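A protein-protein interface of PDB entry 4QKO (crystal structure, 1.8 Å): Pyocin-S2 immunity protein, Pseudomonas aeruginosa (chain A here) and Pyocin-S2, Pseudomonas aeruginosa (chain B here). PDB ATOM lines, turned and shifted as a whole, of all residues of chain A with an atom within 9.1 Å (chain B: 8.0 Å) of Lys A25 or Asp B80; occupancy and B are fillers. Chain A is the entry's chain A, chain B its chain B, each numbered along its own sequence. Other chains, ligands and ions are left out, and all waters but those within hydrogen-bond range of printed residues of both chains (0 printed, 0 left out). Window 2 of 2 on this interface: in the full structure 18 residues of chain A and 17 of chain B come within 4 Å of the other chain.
Among the printed residues, merely in contact across the chains: Thr A22 with Ala B76, Asn A23 with Val B77, Glu A31 with Gly B82, Glu A31 with Ala B83 and His A34 with Val B77.
The backbone NH of Gly B82 lies within hydrogen-bond range of the backbone carbonyl oxygen of Val B77, 3.0 Å away. O of Lys A18 lies within hydrogen-bond range of OG1 of Thr A22, 2.6 Å away. A ring nitrogen (NE2) of His A34 sits at hydrogen-bond distance from the backbone carbonyl oxygen of Ile A20 (2.8 Å). The side-chain amino group of Lys A25 sits at hydrogen-bond distance from the backbone carbonyl oxygen of Phe A28 (3.3 Å). O of Pro A29 lies within hydrogen-bond range of NZ of Lys A25 (2.8 Å).
Of chain B, only Asp B80 (2.5 Å) comes within 4 Å of Lys A25. No residue of chain A comes within 4 Å of Gly B81. Of the printed residues of chain B, Glu A31 touches Arg B53, Gly B82 and Ala B83. Of the printed residues of chain B, Asn A23 touches Ala B76, Val B77 and Asp B80. Of the printed residues of chain B, His A34 touches Val B77 (3.7 Å). Printed residues of chain A within 4 Å of Arg B53: Glu A31. Glu B54 touches none of the printed residues of chain A. Met B78 touches none of the printed residues of chain A. The nearest residue of chain B that does not touch Lys A25 is Ala B76 (6.5 Å).
Of the 16 printed residues of chain B, 6 touch a printed residue of chain A. Hydrophobic or aromatic side chains of chain B within 4 Å of the printed part of chain A: Ala B76 and Val B77. Hydrophobic or aromatic side chains of chain A that line the printed part of chain B: His A34. Among the printed residues, Asp or Glu carboxylates within 4 Å of a Lys or Arg side-chain nitrogen of the other chain: Lys A25 with Asp B80 (2.5 Å) and Glu A31 with Arg B53 (2.7 Å).
OE2 of Glu A31 is in salt-bridge range of NH2 of Arg B53 (2.7 Å). The side-chain amide oxygen (OD1) of Asn A23 sits close to the backbone carbonyl oxygen (O) of Ala B76, at 3.1 Å. The side-chain amide oxygen (OD1) of Asn A23 lies close to the side-chain carboxylate (OD2) of Asp B80, 3.3 Å away. NZ of Lys A25 lies within salt-bridge range of OD2 of Asp B80 (2.5 Å).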
ATOM      1  N   LYS A  18      11.059 -12.705  -5.553  1.00  0.00           N
ATOM      2  CA  LYS A  18      10.703 -13.795  -4.643  1.00  0.00           C
ATOM      3  C   LYS A  18      11.407 -15.053  -5.093  1.00  0.00           C
ATOM      4  O   LYS A  18      11.906 -15.800  -4.238  1.00  0.00           O
ATOM      5  CB  LYS A  18       9.224 -14.176  -4.641  1.00  0.00           C
ATOM      6  CG  LYS A  18       8.196 -13.434  -3.811  1.00  0.00           C
ATOM      7  CD  LYS A  18       6.872 -14.216  -3.907  1.00  0.00           C
ATOM      8  CE  LYS A  18       5.618 -13.329  -3.985  1.00  0.00           C
ATOM      9  NZ  LYS A  18       5.141 -12.921  -2.637  1.00  0.00           N
ATOM     10  N   ASP A  19      11.465 -15.299  -6.407  1.00  0.00           N
ATOM     11  CA  ASP A  19      12.205 -16.459  -6.929  1.00  0.00           C
ATOM     12  C   ASP A  19      13.671 -16.465  -6.587  1.00  0.00           C
ATOM     13  O   ASP A  19      14.226 -17.507  -6.192  1.00  0.00           O
ATOM     14  CB  ASP A  19      12.036 -16.636  -8.438  1.00  0.00           C
ATOM     15  CG  ASP A  19      10.584 -17.081  -8.826  1.00  0.00           C
ATOM     16  OD1 ASP A  19       9.895 -17.705  -7.984  1.00  0.00           O
ATOM     17  OD2 ASP A  19      10.128 -16.786  -9.972  1.00  0.00           O
ATOM     18  N   ILE A  20      14.313 -15.316  -6.759  1.00  0.00           N
ATOM     19  CA  ILE A  20      15.728 -15.209  -6.357  1.00  0.00           C
ATOM     20  C   ILE A  20      15.884 -15.405  -4.846  1.00  0.00           C
ATOM     21  O   ILE A  20      16.718 -16.209  -4.401  1.00  0.00           O
ATOM     22  CB  ILE A  20      16.324 -13.824  -6.726  1.00  0.00           C
ATOM     23  CG1 ILE A  20      16.342 -13.686  -8.227  1.00  0.00           C
ATOM     24  CG2 ILE A  20      17.704 -13.696  -6.119  1.00  0.00           C
ATOM     25  CD1 ILE A  20      16.831 -12.351  -8.778  1.00  0.00           C
ATOM     26  N   THR A  22      13.936 -16.733  -2.426  1.00  0.00           N
ATOM     27  CA  THR A  22      13.614 -18.052  -1.886  1.00  0.00           C
ATOM     28  C   THR A  22      14.428 -19.156  -2.519  1.00  0.00           C
ATOM     29  O   THR A  22      14.273 -20.334  -2.131  1.00  0.00           O
ATOM     30  CB  THR A  22      12.099 -18.397  -2.094  1.00  0.00           C
ATOM     31  OG1 THR A  22      11.772 -18.254  -3.483  1.00  0.00           O
ATOM     32  CG2 THR A  22      11.258 -17.437  -1.267  1.00  0.00           C
ATOM     33  N   ASN A  23      15.259 -18.830  -3.496  1.00  0.00           N
ATOM     34  CA  ASN A  23      16.005 -19.822  -4.240  1.00  0.00           C
ATOM     35  C   ASN A  23      15.073 -20.917  -4.822  1.00  0.00           C
ATOM     36  O   ASN A  23      15.227 -22.126  -4.560  1.00  0.00           O
ATOM     37  CB  ASN A  23      17.116 -20.437  -3.378  1.00  0.00           C
ATOM     38  CG  ASN A  23      18.056 -21.311  -4.158  1.00  0.00           C
ATOM     39  OD1 ASN A  23      18.658 -22.257  -3.601  1.00  0.00           O
ATOM     40  ND2 ASN A  23      18.205 -21.042  -5.428  1.00  0.00           N
ATOM     41  N   ASN A  24      14.139 -20.452  -5.612  1.00  0.00           N
ATOM     42  CA  ASN A  24      13.201 -21.306  -6.336  1.00  0.00           C
ATOM     43  C   ASN A  24      13.962 -22.138  -7.379  1.00  0.00           C
ATOM     44  O   ASN A  24      14.400 -21.596  -8.361  1.00  0.00           O
ATOM     45  CB  ASN A  24      12.199 -20.439  -7.060  1.00  0.00           C
ATOM     46  CG  ASN A  24      11.138 -21.271  -7.803  1.00  0.00           C
ATOM     47  OD1 ASN A  24      11.294 -22.445  -8.004  1.00  0.00           O
ATOM     48  ND2 ASN A  24      10.065 -20.660  -8.135  1.00  0.00           N
ATOM     49  N   LYS A  25      14.126 -23.442  -7.145  1.00  0.00           N
ATOM     50  CA  LYS A  25      14.908 -24.286  -8.014  1.00  0.00           C
ATOM     51  C   LYS A  25      14.249 -24.602  -9.341  1.00  0.00           C
ATOM     52  O   LYS A  25      14.928 -24.938 -10.297  1.00  0.00           O
ATOM     53  CB  LYS A  25      15.215 -25.617  -7.322  1.00  0.00           C
ATOM     54  CG  LYS A  25      15.986 -25.470  -6.016  1.00  0.00           C
ATOM     55  CD  LYS A  25      17.304 -24.765  -6.195  1.00  0.00           C
ATOM     56  CE  LYS A  25      18.296 -25.659  -6.908  1.00  0.00           C
ATOM     57  NZ  LYS A  25      19.640 -25.003  -7.042  1.00  0.00           N
ATOM     58  N   LYS A  26      12.934 -24.477  -9.413  1.00  0.00           N
ATOM     59  CA  LYS A  26      12.283 -24.626 -10.690  1.00  0.00           C
ATOM     60  C   LYS A  26      12.753 -23.539 -11.660  1.00  0.00           C
ATOM     61  O   LYS A  26      12.902 -23.803 -12.862  1.00  0.00           O
ATOM     62  CB  LYS A  26      10.777 -24.621 -10.534  1.00  0.00           C
ATOM     63  CG  LYS A  26      10.087 -24.686 -11.883  1.00  0.00           C
ATOM     64  CD  LYS A  26       8.899 -25.605 -11.824  1.00  0.00           C
ATOM     65  CE  LYS A  26       7.699 -24.870 -11.296  1.00  0.00           C
ATOM     66  NZ  LYS A  26       6.805 -24.583 -12.438  1.00  0.00           N
ATOM     67  N   LYS A  27      13.027 -22.322 -11.137  1.00  0.00           N
ATOM     68  CA  LYS A  27      13.509 -21.221 -11.961  1.00  0.00           C
ATOM     69  C   LYS A  27      15.027 -21.199 -12.113  1.00  0.00           C
ATOM     70  O   LYS A  27      15.529 -20.873 -13.178  1.00  0.00           O
ATOM     71  CB  LYS A  27      13.087 -19.858 -11.370  1.00  0.00           C
ATOM     72  CG  LYS A  27      11.583 -19.645 -11.176  1.00  0.00           C
ATOM     73  CD  LYS A  27      10.808 -19.563 -12.491  1.00  0.00           C
ATOM     74  CE  LYS A  27       9.816 -18.372 -12.554  1.00  0.00           C
ATOM     75  NZ  LYS A  27       8.758 -18.326 -11.478  1.00  0.00           N
ATOM     76  N   PHE A  28      15.723 -21.522 -11.026  1.00  0.00           N
ATOM     77  CA  PHE A  28      17.182 -21.547 -10.923  1.00  0.00           C
ATOM     78  C   PHE A  28      17.673 -22.908 -10.428  1.00  0.00           C
ATOM     79  O   PHE A  28      18.085 -23.058  -9.247  1.00  0.00           O
ATOM     80  CB  PHE A  28      17.599 -20.448  -9.962  1.00  0.00           C
ATOM     81  CG  PHE A  28      16.955 -19.154 -10.287  1.00  0.00           C
ATOM     82  CD1 PHE A  28      17.194 -18.572 -11.516  1.00  0.00           C
ATOM     83  CD2 PHE A  28      16.078 -18.560  -9.403  1.00  0.00           C
ATOM     84  CE1 PHE A  28      16.590 -17.385 -11.848  1.00  0.00           C
ATOM     85  CE2 PHE A  28      15.498 -17.368  -9.703  1.00  0.00           C
ATOM     86  CZ  PHE A  28      15.724 -16.796 -10.946  1.00  0.00           C
ATOM     87  N   PRO A  29      17.645 -23.925 -11.334  1.00  0.00           N
ATOM     88  CA  PRO A  29      17.989 -25.255 -10.898  1.00  0.00           C
ATOM     89  C   PRO A  29      19.465 -25.348 -10.471  1.00  0.00           C
ATOM     90  O   PRO A  29      19.778 -26.144  -9.596  1.00  0.00           O
ATOM     91  CB  PRO A  29      17.760 -26.128 -12.129  1.00  0.00           C
ATOM     92  CG  PRO A  29      17.307 -25.278 -13.210  1.00  0.00           C
ATOM     93  CD  PRO A  29      17.258 -23.854 -12.742  1.00  0.00           C
ATOM     94  N   THR A  30      20.341 -24.570 -11.119  1.00  0.00           N
ATOM     95  CA  THR A  30      21.776 -24.551 -10.807  1.00  0.00           C
ATOM     96  C   THR A  30      22.237 -23.263 -10.096  1.00  0.00           C
ATOM     97  O   THR A  30      21.638 -22.169 -10.297  1.00  0.00           O
ATOM     98  CB  THR A  30      22.586 -24.609 -12.092  1.00  0.00           C
ATOM     99  OG1 THR A  30      22.308 -23.480 -12.889  1.00  0.00           O
ATOM    100  CG2 THR A  30      22.287 -25.916 -12.907  1.00  0.00           C
ATOM    101  N   GLU A  31      23.327 -23.390  -9.333  1.00  0.00           N
ATOM    102  CA  GLU A  31      23.933 -22.269  -8.650  1.00  0.00           C
ATOM    103  C   GLU A  31      24.330 -21.196  -9.662  1.00  0.00           C
ATOM    104  O   GLU A  31      24.153 -19.977  -9.416  1.00  0.00           O
ATOM    105  CB  GLU A  31      25.141 -22.696  -7.775  1.00  0.00           C
ATOM    106  CG  GLU A  31      25.684 -21.567  -6.926  1.00  0.00           C
ATOM    107  CD  GLU A  31      26.798 -21.973  -5.967  1.00  0.00           C
ATOM    108  OE1 GLU A  31      27.202 -23.155  -5.943  1.00  0.00           O
ATOM    109  OE2 GLU A  31      27.315 -21.100  -5.244  1.00  0.00           O
ATOM    110  N   GLU A  32      24.803 -21.651 -10.811  1.00  0.00           N
ATOM    111  CA  GLU A  32      25.200 -20.744 -11.914  1.00  0.00           C
ATOM    112  C   GLU A  32      24.019 -19.957 -12.475  1.00  0.00           C
ATOM    113  O   GLU A  32      24.173 -18.776 -12.827  1.00  0.00           O
ATOM    114  CB  GLU A  32      25.897 -21.531 -13.037  1.00  0.00           C
ATOM    115  CG  GLU A  32      27.233 -22.182 -12.623  1.00  0.00           C
ATOM    116  CD  GLU A  32      27.147 -23.488 -11.753  1.00  0.00           C
ATOM    117  OE1 GLU A  32      26.064 -24.123 -11.552  1.00  0.00           O
ATOM    118  OE2 GLU A  32      28.208 -23.891 -11.228  1.00  0.00           O
ATOM    119  N   SER A  33      22.836 -20.600 -12.543  1.00  0.00           N
ATOM    120  CA  SER A  33      21.627 -19.922 -12.980  1.00  0.00           C
ATOM    121  C   SER A  33      21.184 -18.870 -11.959  1.00  0.00           C
ATOM    122  O   SER A  33      20.681 -17.784 -12.330  1.00  0.00           O
ATOM    123  CB  SER A  33      20.436 -20.857 -13.222  1.00  0.00           C
ATOM    124  OG  SER A  33      19.939 -21.451 -12.032  1.00  0.00           O
ATOM    125  N   HIS A  34      21.329 -19.188 -10.671  1.00  0.00           N
ATOM    126  CA  HIS A  34      20.976 -18.214  -9.642  1.00  0.00           C
ATOM    127  C   HIS A  34      21.903 -17.002  -9.681  1.00  0.00           C
ATOM    128  O   HIS A  34      21.458 -15.860  -9.488  1.00  0.00           O
ATOM    129  CB  HIS A  34      21.058 -18.870  -8.249  1.00  0.00           C
ATOM    130  CG  HIS A  34      20.392 -18.097  -7.185  1.00  0.00           C
ATOM    131  ND1 HIS A  34      21.079 -17.178  -6.418  1.00  0.00           N
ATOM    132  CD2 HIS A  34      19.116 -18.094  -6.738  1.00  0.00           C
ATOM    133  CE1 HIS A  34      20.247 -16.642  -5.546  1.00  0.00           C
ATOM    134  NE2 HIS A  34      19.045 -17.184  -5.709  1.00  0.00           N
ATOM    135  N   ILE A  35      23.184 -17.237  -9.868  1.00  0.00           N
ATOM    136  CA  ILE A  35      24.131 -16.140  -9.914  1.00  0.00           C
ATOM    137  C   ILE A  35      23.768 -15.192 -11.035  1.00  0.00           C
ATOM    138  O   ILE A  35      23.807 -13.949 -10.864  1.00  0.00           O
ATOM    139  CB  ILE A  35      25.600 -16.616 -10.037  1.00  0.00           C
ATOM    140  CG1 ILE A  35      26.082 -17.258  -8.734  1.00  0.00           C
ATOM    141  CG2 ILE A  35      26.518 -15.434 -10.373  1.00  0.00           C
ATOM    142  CD1 ILE A  35      27.358 -18.081  -8.810  1.00  0.00           C
ATOM    143  N   ARG B  53      32.144 -28.625  -0.530  1.00  0.00           N
ATOM    144  CA  ARG B  53      31.627 -27.240  -0.431  1.00  0.00           C
ATOM    145  C   ARG B  53      30.130 -27.229  -0.161  1.00  0.00           C
ATOM    146  O   ARG B  53      29.623 -26.478   0.682  1.00  0.00           O
ATOM    147  CB  ARG B  53      31.976 -26.493  -1.722  1.00  0.00           C
ATOM    148  CG  ARG B  53      31.575 -25.022  -1.787  1.00  0.00           C
ATOM    149  CD  ARG B  53      31.880 -24.505  -3.195  1.00  0.00           C
ATOM    150  NE  ARG B  53      31.341 -23.214  -3.434  1.00  0.00           N
ATOM    151  CZ  ARG B  53      30.117 -22.984  -3.921  1.00  0.00           C
ATOM    152  NH1 ARG B  53      29.284 -23.994  -4.228  1.00  0.00           N
ATOM    153  NH2 ARG B  53      29.718 -21.740  -4.080  1.00  0.00           N
ATOM    154  N   GLU B  54      29.441 -28.085  -0.871  1.00  0.00           N
ATOM    155  CA  GLU B  54      28.044 -28.295  -0.659  1.00  0.00           C
ATOM    156  C   GLU B  54      27.733 -28.751   0.773  1.00  0.00           C
ATOM    157  O   GLU B  54      26.915 -28.167   1.430  1.00  0.00           O
ATOM    158  CB  GLU B  54      27.511 -29.333  -1.612  1.00  0.00           C
ATOM    159  CG  GLU B  54      27.259 -28.812  -2.979  1.00  0.00           C
ATOM    160  CD  GLU B  54      26.758 -29.930  -3.903  1.00  0.00           C
ATOM    161  OE1 GLU B  54      26.354 -31.032  -3.390  1.00  0.00           O
ATOM    162  OE2 GLU B  54      26.801 -29.678  -5.132  1.00  0.00           O
ATOM    163  N   GLN B  55      28.411 -29.771   1.266  1.00  0.00           N
ATOM    164  CA  GLN B  55      28.199 -30.193   2.647  1.00  0.00           C
ATOM    165  C   GLN B  55      28.605 -29.180   3.658  1.00  0.00           C
ATOM    166  O   GLN B  55      27.971 -29.082   4.674  1.00  0.00           O
ATOM    167  CB  GLN B  55      28.909 -31.519   2.919  1.00  0.00           C
ATOM    168  CG  GLN B  55      28.166 -32.631   2.165  1.00  0.00           C
ATOM    169  CD  GLN B  55      28.856 -33.991   2.337  1.00  0.00           C
ATOM    170  OE1 GLN B  55      29.225 -34.389   3.452  1.00  0.00           O
ATOM    171  NE2 GLN B  55      29.060 -34.707   1.215  1.00  0.00           N
ATOM    172  N   TRP B  57      28.473 -25.700   3.342  1.00  0.00           N
ATOM    173  CA  TRP B  57      27.441 -24.681   3.501  1.00  0.00           C
ATOM    174  C   TRP B  57      26.086 -25.194   4.018  1.00  0.00           C
ATOM    175  O   TRP B  57      25.367 -24.512   4.698  1.00  0.00           O
ATOM    176  CB  TRP B  57      27.267 -23.867   2.204  1.00  0.00           C
ATOM    177  CG  TRP B  57      28.493 -23.083   1.973  1.00  0.00           C
ATOM    178  CD1 TRP B  57      29.360 -23.277   0.975  1.00  0.00           C
ATOM    179  CD2 TRP B  57      29.005 -21.997   2.749  1.00  0.00           C
ATOM    180  NE1 TRP B  57      30.446 -22.387   1.096  1.00  0.00           N
ATOM    181  CE2 TRP B  57      30.190 -21.559   2.140  1.00  0.00           C
ATOM    182  CE3 TRP B  57      28.563 -21.328   3.890  1.00  0.00           C
ATOM    183  CZ2 TRP B  57      30.956 -20.508   2.662  1.00  0.00           C
ATOM    184  CZ3 TRP B  57      29.315 -20.289   4.394  1.00  0.00           C
ATOM    185  CH2 TRP B  57      30.462 -19.894   3.822  1.00  0.00           C
ATOM    186  N   ILE B  58      25.758 -26.441   3.731  1.00  0.00           N
ATOM    187  CA  ILE B  58      24.534 -27.010   4.336  1.00  0.00           C
ATOM    188  C   ILE B  58      24.674 -27.107   5.855  1.00  0.00           C
ATOM    189  O   ILE B  58      23.751 -26.757   6.579  1.00  0.00           O
ATOM    190  CB  ILE B  58      24.199 -28.385   3.711  1.00  0.00           C
ATOM    191  CG1 ILE B  58      23.626 -28.173   2.293  1.00  0.00           C
ATOM    192  CG2 ILE B  58      23.232 -29.149   4.602  1.00  0.00           C
ATOM    193  CD1 ILE B  58      23.913 -29.353   1.346  1.00  0.00           C
ATOM    194  N   ALA B  61      24.263 -23.644   7.390  1.00  0.00           N
ATOM    195  CA  ALA B  61      22.869 -23.214   7.348  1.00  0.00           C
ATOM    196  C   ALA B  61      21.979 -23.938   8.400  1.00  0.00           C
ATOM    197  O   ALA B  61      21.026 -23.340   8.916  1.00  0.00           O
ATOM    198  CB  ALA B  61      22.297 -23.408   5.953  1.00  0.00           C
ATOM    199  N   SER B  74      19.923 -15.544   2.226  1.00  0.00           N
ATOM    200  CA  SER B  74      21.171 -16.274   2.213  1.00  0.00           C
ATOM    201  C   SER B  74      20.990 -17.755   2.604  1.00  0.00           C
ATOM    202  O   SER B  74      21.624 -18.653   2.028  1.00  0.00           O
ATOM    203  CB  SER B  74      22.125 -15.608   3.186  1.00  0.00           C
ATOM    204  OG  SER B  74      22.657 -14.392   2.676  1.00  0.00           O
ATOM    205  N   LEU B  75      20.147 -18.024   3.579  1.00  0.00           N
ATOM    206  CA  LEU B  75      19.961 -19.391   3.992  1.00  0.00           C
ATOM    207  C   LEU B  75      19.319 -20.216   2.892  1.00  0.00           C
ATOM    208  O   LEU B  75      19.582 -21.429   2.755  1.00  0.00           O
ATOM    209  CB  LEU B  75      19.166 -19.436   5.249  1.00  0.00           C
ATOM    210  CG  LEU B  75      19.841 -18.873   6.480  1.00  0.00           C
ATOM    211  CD1 LEU B  75      18.866 -18.662   7.588  1.00  0.00           C
ATOM    212  CD2 LEU B  75      20.977 -19.834   6.842  1.00  0.00           C
ATOM    213  N   ALA B  76      18.485 -19.589   2.102  1.00  0.00           N
ATOM    214  CA  ALA B  76      17.818 -20.285   1.014  1.00  0.00           C
ATOM    215  C   ALA B  76      18.856 -20.800   0.022  1.00  0.00           C
ATOM    216  O   ALA B  76      18.727 -21.919  -0.496  1.00  0.00           O
ATOM    217  CB  ALA B  76      16.781 -19.374   0.354  1.00  0.00           C
ATOM    218  N   VAL B  77      19.970 -20.082  -0.112  1.00  0.00           N
ATOM    219  CA  VAL B  77      21.063 -20.472  -0.976  1.00  0.00           C
ATOM    220  C   VAL B  77      21.915 -21.549  -0.266  1.00  0.00           C
ATOM    221  O   VAL B  77      22.262 -22.566  -0.888  1.00  0.00           O
ATOM    222  CB  VAL B  77      21.924 -19.233  -1.351  1.00  0.00           C
ATOM    223  CG1 VAL B  77      23.263 -19.661  -1.904  1.00  0.00           C
ATOM    224  CG2 VAL B  77      21.164 -18.382  -2.362  1.00  0.00           C
ATOM    225  N   MET B  78      22.171 -21.360   1.026  1.00  0.00           N
ATOM    226  CA  MET B  78      23.112 -22.202   1.733  1.00  0.00           C
ATOM    227  C   MET B  78      22.540 -23.598   2.015  1.00  0.00           C
ATOM    228  O   MET B  78      23.267 -24.603   1.986  1.00  0.00           O
ATOM    229  CB  MET B  78      23.537 -21.509   3.034  1.00  0.00           C
ATOM    230  CG  MET B  78      24.463 -20.324   2.771  1.00  0.00           C
ATOM    231  SD  MET B  78      24.269 -19.055   4.056  1.00  0.00           S
ATOM    232  CE  MET B  78      25.217 -19.951   5.212  1.00  0.00           C
ATOM    233  N   ARG B  79      21.231 -23.642   2.245  1.00  0.00           N
ATOM    234  CA  ARG B  79      20.543 -24.926   2.467  1.00  0.00           C
ATOM    235  C   ARG B  79      20.652 -25.825   1.304  1.00  0.00           C
ATOM    236  O   ARG B  79      20.536 -27.045   1.482  1.00  0.00           O
ATOM    237  CB  ARG B  79      19.055 -24.710   2.657  1.00  0.00           C
ATOM    238  CG  ARG B  79      18.748 -24.365   4.042  1.00  0.00           C
ATOM    239  CD  ARG B  79      17.247 -24.151   4.167  1.00  0.00           C
ATOM    240  NE  ARG B  79      17.112 -23.346   5.364  1.00  0.00           N
ATOM    241  CZ  ARG B  79      16.580 -22.136   5.455  1.00  0.00           C
ATOM    242  NH1 ARG B  79      16.011 -21.530   4.404  1.00  0.00           N
ATOM    243  NH2 ARG B  79      16.599 -21.550   6.645  1.00  0.00           N
ATOM    244  N   ASP B  80      20.880 -25.235   0.130  1.00  0.00           N
ATOM    245  CA  ASP B  80      20.947 -25.930  -1.159  1.00  0.00           C
ATOM    246  C   ASP B  80      22.409 -26.263  -1.518  1.00  0.00           C
ATOM    247  O   ASP B  80      22.699 -26.774  -2.623  1.00  0.00           O
ATOM    248  CB  ASP B  80      20.294 -24.991  -2.205  1.00  0.00           C
ATOM    249  CG  ASP B  80      20.121 -25.616  -3.618  1.00  0.00           C
ATOM    250  OD1 ASP B  80      19.613 -26.769  -3.742  1.00  0.00           O
ATOM    251  OD2 ASP B  80      20.420 -24.891  -4.632  1.00  0.00           O
ATOM    252  N   GLY B  81      23.327 -25.958  -0.602  1.00  0.00           N
ATOM    253  CA  GLY B  81      24.731 -26.201  -0.825  1.00  0.00           C
ATOM    254  C   GLY B  81      25.495 -25.037  -1.399  1.00  0.00           C
ATOM    255  O   GLY B  81      26.672 -25.161  -1.688  1.00  0.00           O
ATOM    256  N   GLY B  82      24.843 -23.892  -1.574  1.00  0.00           N
ATOM    257  CA  GLY B  82      25.573 -22.782  -2.230  1.00  0.00           C
ATOM    258  C   GLY B  82      26.220 -21.890  -1.165  1.00  0.00           C
ATOM    259  O   GLY B  82      25.726 -21.802  -0.087  1.00  0.00           O
ATOM    260  N   ALA B  83      27.360 -21.286  -1.478  1.00  0.00           N
ATOM    261  CA  ALA B  83      27.987 -20.296  -0.623  1.00  0.00           C
ATOM    262  C   ALA B  83      27.148 -19.032  -0.630  1.00  0.00           C
ATOM    263  O   ALA B  83      26.586 -18.673  -1.642  1.00  0.00           O
ATOM    264  CB  ALA B  83      29.382 -19.946  -1.145  1.00  0.00           C
